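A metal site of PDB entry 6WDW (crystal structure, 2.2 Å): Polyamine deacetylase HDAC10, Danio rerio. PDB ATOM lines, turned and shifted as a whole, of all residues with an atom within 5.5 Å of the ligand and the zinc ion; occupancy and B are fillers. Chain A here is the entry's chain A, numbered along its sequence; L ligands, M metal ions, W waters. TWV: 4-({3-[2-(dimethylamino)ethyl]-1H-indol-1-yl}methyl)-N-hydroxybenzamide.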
ATOM      1  N   PRO A  23      -8.370  25.880  -4.412  1.00  0.00           N
ATOM      2  CA  PRO A  23      -6.957  26.147  -4.120  1.00  0.00           C
ATOM      3  C   PRO A  23      -6.074  24.946  -4.397  1.00  0.00           C
ATOM      4  O   PRO A  23      -4.871  25.134  -4.663  1.00  0.00           O
ATOM      5  CB  PRO A  23      -6.957  26.506  -2.632  1.00  0.00           C
ATOM      6  CG  PRO A  23      -8.423  26.664  -2.247  1.00  0.00           C
ATOM      7  CD  PRO A  23      -9.190  25.798  -3.191  1.00  0.00           C
ATOM      8  N   GLU A  24      -6.610  23.730  -4.361  1.00  0.00           N
ATOM      9  CA  GLU A  24      -5.817  22.553  -4.691  1.00  0.00           C
ATOM     10  C   GLU A  24      -5.465  22.508  -6.176  1.00  0.00           C
ATOM     11  O   GLU A  24      -4.359  22.081  -6.555  1.00  0.00           O
ATOM     12  CB  GLU A  24      -6.578  21.278  -4.309  1.00  0.00           C
ATOM     13  CG  GLU A  24      -6.773  21.076  -2.829  1.00  0.00           C
ATOM     14  CD  GLU A  24      -7.058  19.640  -2.486  1.00  0.00           C
ATOM     15  OE1 GLU A  24      -7.177  18.820  -3.439  1.00  0.00           O
ATOM     16  OE2 GLU A  24      -7.142  19.317  -1.286  1.00  0.00           O
ATOM     17  N   CYS A  25      -6.403  22.927  -7.026  1.00  0.00           N
ATOM     18  CA  CYS A  25      -6.290  22.710  -8.459  1.00  0.00           C
ATOM     19  C   CYS A  25      -5.650  23.868  -9.197  1.00  0.00           C
ATOM     20  O   CYS A  25      -5.095  23.675 -10.276  1.00  0.00           O
ATOM     21  CB  CYS A  25      -7.688  22.468  -9.050  1.00  0.00           C
ATOM     22  SG  CYS A  25      -8.244  20.754  -8.848  1.00  0.00           S
ATOM     23  N   ILE A  27      -3.039  25.344  -9.171  1.00  0.00           N
ATOM     24  CA  ILE A  27      -1.628  25.323  -9.508  1.00  0.00           C
ATOM     25  C   ILE A  27      -1.388  24.780 -10.908  1.00  0.00           C
ATOM     26  O   ILE A  27      -0.316  24.991 -11.470  1.00  0.00           O
ATOM     27  CB  ILE A  27      -0.811  24.486  -8.506  1.00  0.00           C
ATOM     28  CG1 ILE A  27      -1.160  22.999  -8.687  1.00  0.00           C
ATOM     29  CG2 ILE A  27      -1.082  24.960  -7.087  1.00  0.00           C
ATOM     30  CD1 ILE A  27      -0.660  22.101  -7.572  1.00  0.00           C
ATOM     31  N   ALA A  94      -9.054  15.815  -6.479  1.00  0.00           N
ATOM     32  CA  ALA A  94      -8.036  16.763  -6.955  1.00  0.00           C
ATOM     33  C   ALA A  94      -7.930  16.769  -8.485  1.00  0.00           C
ATOM     34  O   ALA A  94      -6.864  16.602  -9.080  1.00  0.00           O
ATOM     35  CB  ALA A  94      -6.691  16.451  -6.316  1.00  0.00           C
ATOM     36  N   HIS A 136      -0.115  10.241 -14.637  1.00  0.00           N
ATOM     37  CA  HIS A 136       0.282   9.068 -13.860  1.00  0.00           C
ATOM     38  C   HIS A 136      -0.606   8.797 -12.642  1.00  0.00           C
ATOM     39  O   HIS A 136      -0.470   7.714 -12.070  1.00  0.00           O
ATOM     40  CB  HIS A 136       1.774   9.145 -13.406  1.00  0.00           C
ATOM     41  CG  HIS A 136       2.071  10.205 -12.385  1.00  0.00           C
ATOM     42  ND1 HIS A 136       3.186  10.156 -11.577  1.00  0.00           N
ATOM     43  CD2 HIS A 136       1.409  11.336 -12.054  1.00  0.00           C
ATOM     44  CE1 HIS A 136       3.215  11.221 -10.796  1.00  0.00           C
ATOM     45  NE2 HIS A 136       2.137  11.955 -11.066  1.00  0.00           N
ATOM     46  N   HIS A 137      -1.505   9.697 -12.265  1.00  0.00           N
ATOM     47  CA  HIS A 137      -2.485   9.405 -11.219  1.00  0.00           C
ATOM     48  C   HIS A 137      -3.751   8.745 -11.739  1.00  0.00           C
ATOM     49  O   HIS A 137      -4.512   8.191 -10.922  1.00  0.00           O
ATOM     50  CB  HIS A 137      -2.917  10.670 -10.476  1.00  0.00           C
ATOM     51  CG  HIS A 137      -1.818  11.331  -9.723  1.00  0.00           C
ATOM     52  ND1 HIS A 137      -0.941  10.638  -8.917  1.00  0.00           N
ATOM     53  CD2 HIS A 137      -1.418  12.630  -9.681  1.00  0.00           C
ATOM     54  CE1 HIS A 137      -0.054  11.473  -8.398  1.00  0.00           C
ATOM     55  NE2 HIS A 137      -0.321  12.688  -8.850  1.00  0.00           N
ATOM     56  N   GLY A 145      -5.982  13.643  -9.453  1.00  0.00           N
ATOM     57  CA  GLY A 145      -4.776  14.455  -9.385  1.00  0.00           C
ATOM     58  C   GLY A 145      -4.379  15.100 -10.699  1.00  0.00           C
ATOM     59  O   GLY A 145      -3.281  14.855 -11.206  1.00  0.00           O
ATOM     60  N   PHE A 146      -5.284  15.902 -11.274  1.00  0.00           N
ATOM     61  CA  PHE A 146      -5.176  16.598 -12.557  1.00  0.00           C
ATOM     62  C   PHE A 146      -5.118  15.653 -13.748  1.00  0.00           C
ATOM     63  O   PHE A 146      -5.127  16.126 -14.880  1.00  0.00           O
ATOM     64  CB  PHE A 146      -3.960  17.554 -12.638  1.00  0.00           C
ATOM     65  CG  PHE A 146      -3.757  18.391 -11.413  1.00  0.00           C
ATOM     66  CD1 PHE A 146      -4.828  18.968 -10.772  1.00  0.00           C
ATOM     67  CD2 PHE A 146      -2.481  18.601 -10.890  1.00  0.00           C
ATOM     68  CE1 PHE A 146      -4.641  19.726  -9.617  1.00  0.00           C
ATOM     69  CE2 PHE A 146      -2.294  19.355  -9.772  1.00  0.00           C
ATOM     70  CZ  PHE A 146      -3.383  19.917  -9.121  1.00  0.00           C
ATOM     71  N   ASP A 174       8.583  12.140 -10.873  1.00  0.00           N
ATOM     72  CA  ASP A 174       7.678  13.128 -10.302  1.00  0.00           C
ATOM     73  C   ASP A 174       7.727  13.008  -8.785  1.00  0.00           C
ATOM     74  O   ASP A 174       8.135  11.982  -8.221  1.00  0.00           O
ATOM     75  CB  ASP A 174       6.255  12.884 -10.831  1.00  0.00           C
ATOM     76  CG  ASP A 174       5.274  13.982 -10.468  1.00  0.00           C
ATOM     77  OD1 ASP A 174       4.958  14.816 -11.335  1.00  0.00           O
ATOM     78  OD2 ASP A 174       4.777  14.012  -9.318  1.00  0.00           O
ATOM     79  N   VAL A 175       7.338  14.084  -8.094  1.00  0.00           N
ATOM     80  CA  VAL A 175       7.442  14.066  -6.637  1.00  0.00           C
ATOM     81  C   VAL A 175       6.241  13.398  -5.983  1.00  0.00           C
ATOM     82  O   VAL A 175       6.246  13.169  -4.754  1.00  0.00           O
ATOM     83  CB  VAL A 175       7.607  15.488  -6.056  1.00  0.00           C
ATOM     84  CG1 VAL A 175       6.241  16.161  -5.862  1.00  0.00           C
ATOM     85  CG2 VAL A 175       8.432  15.426  -4.759  1.00  0.00           C
ATOM     86  N   HIS A 176       5.206  13.101  -6.752  1.00  0.00           N
ATOM     87  CA  HIS A 176       4.017  12.412  -6.298  1.00  0.00           C
ATOM     88  C   HIS A 176       4.039  10.966  -6.766  1.00  0.00           C
ATOM     89  O   HIS A 176       4.693  10.658  -7.775  1.00  0.00           O
ATOM     90  CB  HIS A 176       2.770  13.101  -6.824  1.00  0.00           C
ATOM     91  CG  HIS A 176       2.580  14.489  -6.309  1.00  0.00           C
ATOM     92  ND1 HIS A 176       2.983  15.602  -7.012  1.00  0.00           N
ATOM     93  CD2 HIS A 176       1.999  14.953  -5.174  1.00  0.00           C
ATOM     94  CE1 HIS A 176       2.653  16.690  -6.343  1.00  0.00           C
ATOM     95  NE2 HIS A 176       2.062  16.322  -5.216  1.00  0.00           N
ATOM     96  N   TRP A 205      -0.309  13.699   0.199  1.00  0.00           N
ATOM     97  CA  TRP A 205      -1.219  13.238  -0.843  1.00  0.00           C
ATOM     98  C   TRP A 205      -0.453  12.387  -1.852  1.00  0.00           C
ATOM     99  O   TRP A 205       0.683  12.725  -2.214  1.00  0.00           O
ATOM    100  CB  TRP A 205      -1.891  14.449  -1.497  1.00  0.00           C
ATOM    101  CG  TRP A 205      -2.977  14.080  -2.475  1.00  0.00           C
ATOM    102  CD1 TRP A 205      -4.323  14.059  -2.243  1.00  0.00           C
ATOM    103  CD2 TRP A 205      -2.788  13.667  -3.821  1.00  0.00           C
ATOM    104  NE1 TRP A 205      -4.987  13.631  -3.373  1.00  0.00           N
ATOM    105  CE2 TRP A 205      -4.072  13.384  -4.361  1.00  0.00           C
ATOM    106  CE3 TRP A 205      -1.665  13.472  -4.635  1.00  0.00           C
ATOM    107  CZ2 TRP A 205      -4.258  12.935  -5.681  1.00  0.00           C
ATOM    108  CZ3 TRP A 205      -1.844  13.025  -5.939  1.00  0.00           C
ATOM    109  CH2 TRP A 205      -3.138  12.764  -6.446  1.00  0.00           C
ATOM    110  N   ASP A 267       8.091  18.625 -10.375  1.00  0.00           N
ATOM    111  CA  ASP A 267       7.798  19.125  -9.047  1.00  0.00           C
ATOM    112  C   ASP A 267       8.741  18.552  -7.983  1.00  0.00           C
ATOM    113  O   ASP A 267       8.595  18.909  -6.812  1.00  0.00           O
ATOM    114  CB  ASP A 267       6.346  18.845  -8.663  1.00  0.00           C
ATOM    115  CG  ASP A 267       5.874  17.459  -9.036  1.00  0.00           C
ATOM    116  OD1 ASP A 267       6.691  16.535  -9.309  1.00  0.00           O
ATOM    117  OD2 ASP A 267       4.631  17.295  -9.037  1.00  0.00           O
ATOM    118  N   PRO A 273       6.546  24.526  -5.240  1.00  0.00           N
ATOM    119  CA  PRO A 273       5.746  24.687  -4.022  1.00  0.00           C
ATOM    120  C   PRO A 273       5.092  23.403  -3.545  1.00  0.00           C
ATOM    121  O   PRO A 273       4.635  23.356  -2.395  1.00  0.00           O
ATOM    122  CB  PRO A 273       4.707  25.734  -4.423  1.00  0.00           C
ATOM    123  CG  PRO A 273       4.528  25.527  -5.907  1.00  0.00           C
ATOM    124  CD  PRO A 273       5.924  25.187  -6.403  1.00  0.00           C
ATOM    125  N   GLU A 274       5.022  22.362  -4.375  1.00  0.00           N
ATOM    126  CA  GLU A 274       4.384  21.105  -3.993  1.00  0.00           C
ATOM    127  C   GLU A 274       5.352  20.032  -3.531  1.00  0.00           C
ATOM    128  O   GLU A 274       5.072  19.315  -2.557  1.00  0.00           O
ATOM    129  CB  GLU A 274       3.541  20.589  -5.157  1.00  0.00           C
ATOM    130  CG  GLU A 274       2.633  21.675  -5.706  1.00  0.00           C
ATOM    131  CD  GLU A 274       1.472  21.938  -4.772  1.00  0.00           C
ATOM    132  OE1 GLU A 274       0.896  20.940  -4.247  1.00  0.00           O
ATOM    133  OE2 GLU A 274       1.153  23.136  -4.527  1.00  0.00           O
ATOM    134  N   GLU A 276       8.695  20.636  -2.560  1.00  0.00           N
ATOM    135  CA  GLU A 276       9.491  21.209  -1.467  1.00  0.00           C
ATOM    136  C   GLU A 276      10.800  20.449  -1.264  1.00  0.00           C
ATOM    137  O   GLU A 276      11.349  20.402  -0.153  1.00  0.00           O
ATOM    138  CB  GLU A 276       8.687  21.257  -0.165  1.00  0.00           C
ATOM    139  CG  GLU A 276       7.456  22.166  -0.235  1.00  0.00           C
ATOM    140  CD  GLU A 276       6.583  22.076   1.023  1.00  0.00           C
ATOM    141  OE1 GLU A 276       7.143  22.230   2.135  1.00  0.00           O
ATOM    142  OE2 GLU A 276       5.360  21.829   0.911  1.00  0.00           O
ATOM    143  N   GLU A 304       4.992  15.085 -16.655  1.00  0.00           N
ATOM    144  CA  GLU A 304       3.936  14.925 -15.674  1.00  0.00           C
ATOM    145  C   GLU A 304       3.720  16.278 -15.003  1.00  0.00           C
ATOM    146  O   GLU A 304       3.079  17.167 -15.594  1.00  0.00           O
ATOM    147  CB  GLU A 304       4.243  13.777 -14.695  1.00  0.00           C
ATOM    148  CG  GLU A 304       4.398  12.409 -15.383  1.00  0.00           C
ATOM    149  CD  GLU A 304       3.079  11.690 -15.658  1.00  0.00           C
ATOM    150  OE1 GLU A 304       2.000  12.240 -15.329  1.00  0.00           O
ATOM    151  OE2 GLU A 304       3.117  10.558 -16.209  1.00  0.00           O
ATOM    152  N   GLY A 305       4.234  16.494 -13.772  1.00  0.00           N
ATOM    153  CA  GLY A 305       3.996  17.717 -13.044  1.00  0.00           C
ATOM    154  C   GLY A 305       5.182  18.678 -13.067  1.00  0.00           C
ATOM    155  O   GLY A 305       6.202  18.434 -13.712  1.00  0.00           O
ATOM    156  N   GLY A 306       5.028  19.777 -12.338  1.00  0.00           N
ATOM    157  CA  GLY A 306       6.049  20.809 -12.229  1.00  0.00           C
ATOM    158  C   GLY A 306       5.405  22.175 -12.244  1.00  0.00           C
ATOM    159  O   GLY A 306       4.799  22.559 -13.249  1.00  0.00           O
ATOM    160  N   TYR A 307       5.486  22.925 -11.135  1.00  0.00           N
ATOM    161  CA  TYR A 307       4.590  24.036 -10.908  1.00  0.00           C
ATOM    162  C   TYR A 307       5.265  25.369 -10.667  1.00  0.00           C
ATOM    163  O   TYR A 307       4.573  26.395 -10.747  1.00  0.00           O
ATOM    164  CB  TYR A 307       3.660  23.731  -9.723  1.00  0.00           C
ATOM    165  CG  TYR A 307       2.922  22.478  -9.980  1.00  0.00           C
ATOM    166  CD1 TYR A 307       1.902  22.447 -10.907  1.00  0.00           C
ATOM    167  CD2 TYR A 307       3.289  21.290  -9.353  1.00  0.00           C
ATOM    168  CE1 TYR A 307       1.242  21.290 -11.195  1.00  0.00           C
ATOM    169  CE2 TYR A 307       2.628  20.113  -9.631  1.00  0.00           C
ATOM    170  CZ  TYR A 307       1.605  20.123 -10.557  1.00  0.00           C
ATOM    171  OH  TYR A 307       0.901  18.982 -10.866  1.00  0.00           O
HETATM  172  C10 TWV L   1      -2.747  20.276  -4.493  1.00  0.00           C
HETATM  173  C13 TWV L   1      -0.977  22.208  -1.982  1.00  0.00           C
HETATM  174  C15 TWV L   1       1.053  23.425  -1.189  1.00  0.00           C
HETATM  175  C17 TWV L   1      -3.198  19.832  -2.318  1.00  0.00           C
HETATM  176  C20 TWV L   1      -4.257  17.480  -1.101  1.00  0.00           C
HETATM  177  C21 TWV L   1      -3.932  18.616  -0.322  1.00  0.00           C
HETATM  178  C22 TWV L   1      -3.417  19.751  -0.931  1.00  0.00           C
HETATM  179  C24 TWV L   1      -1.366  16.221  -8.240  1.00  0.00           C
HETATM  180  C03 TWV L   1       1.022  16.401  -9.179  1.00  0.00           C
HETATM  181  C04 TWV L   1      -0.148  16.861  -8.303  1.00  0.00           C
HETATM  182  C05 TWV L   1       0.020  17.952  -7.403  1.00  0.00           C
HETATM  183  C06 TWV L   1      -1.027  18.362  -6.543  1.00  0.00           C
HETATM  184  C07 TWV L   1      -2.280  17.694  -6.511  1.00  0.00           C
HETATM  185  C08 TWV L   1      -3.467  18.071  -5.641  1.00  0.00           C
HETATM  186  C11 TWV L   1      -2.700  20.847  -3.245  1.00  0.00           C
HETATM  187  C12 TWV L   1      -2.217  22.228  -2.901  1.00  0.00           C
HETATM  188  C16 TWV L   1      -0.924  24.693  -1.910  1.00  0.00           C
HETATM  189  C18 TWV L   1      -3.549  18.659  -3.092  1.00  0.00           C
HETATM  190  C19 TWV L   1      -4.076  17.506  -2.482  1.00  0.00           C
HETATM  191  C23 TWV L   1      -2.395  16.628  -7.394  1.00  0.00           C
HETATM  192  N02 TWV L   1       0.966  15.011  -9.634  1.00  0.00           N
HETATM  193  N09 TWV L   1      -3.250  18.943  -4.465  1.00  0.00           N
HETATM  194  N14 TWV L   1      -0.110  23.439  -2.162  1.00  0.00           N
HETATM  195  O01 TWV L   1       2.015  14.559 -10.380  1.00  0.00           O
HETATM  196  O25 TWV L   1       1.987  17.053  -9.412  1.00  0.00           O
HETATM  197 ZN    ZN M   1       3.515  15.538  -9.161  1.00  0.00          ZN
HETATM  198  O   HOH W   1      -0.301  18.548  -1.371  1.00  0.00           O
HETATM  199  O   HOH W   2       1.656  20.324  -1.268  1.00  0.00           O
HETATM  200  O   HOH W   3       0.690  18.445  -3.687  1.00  0.00           O
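Water W3 lies within hydrogen-bond range of the side-chain carboxylate (OE1) of Glu 274 and a ring nitrogen (NE2) of His 176.
Of the 21 residues printed, 3 come within 4 Å of the zinc ion.
Residues that only touch the ligand: Glu 24 (3.2 Å), Ile 27 (3.9 Å), Ala 94 (3.7 Å), Gly 145 (3.8 Å), Phe 146 (3.6 Å), Trp 205 (3.5 Å) and Pro 273 (3.8 Å). 14 residues have an atom within 4 Å of the ligand: Glu 24, Ile 27, Ala 94, His 136, His 137, Gly 145, Phe 146, Asp 174, His 176, Trp 205, Asp 267, Pro 273, Glu 274 and Tyr 307. Along chain A the residues within 4 Å of the ligand span positions 24 to 307. The nearest printed residue that does not touch the ligand is Gly 305 (4.2 Å).
The backbone carbonyl oxygen (O) of Ala 94 lies within hydrogen-bond range of the backbone NH (N) of Phe 146, 2.8 Å away. The side-chain carboxylate (OD1) of Asp 174 lies within hydrogen-bond range of the backbone NH (N) of Gly 305 (3.0 Å). NE2 of His 136 is in hydrogen-bond range of NE2 of His 137 (3.4 Å). N of Val 175 sits at hydrogen-bond distance from OD1 of Asp 267. The backbone NH (N) of Gly 145 lies close to the backbone carbonyl oxygen (O) of Ala 94 (3.1 Å). The backbone NH (N) of His 136 lies within hydrogen-bond range of the side-chain carboxylate (OE1) of Glu 304 (3.0 Å).
OE2 of Glu 274 is in salt-bridge range of N14 of the ligand. A ring nitrogen (NE2) of His 136 sits close to an oxygen (O01) of the ligand (2.7 Å). The side-chain hydroxyl of Tyr 307 sits close to an oxygen (O25) of the ligand, 2.6 Å away. A ring nitrogen (NE2) of His 137 lies within hydrogen-bond range of a nitrogen (N02) of the ligand, at 2.8 Å.
The zinc ion is bound by the side-chain carboxylate (OD2) of Asp 174 (2.0 Å), the side-chain carboxylate (OD2) of Asp 267 (2.1 Å), an oxygen (O25) of the ligand (2.2 Å), an oxygen (O01) of the ligand (2.2 Å) and a ring nitrogen (ND1) of His 176 (2.2 Å). Slightly farther from the zinc ion lies the side-chain carboxylate (OD1) of Asp 174 (2.7 Å).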
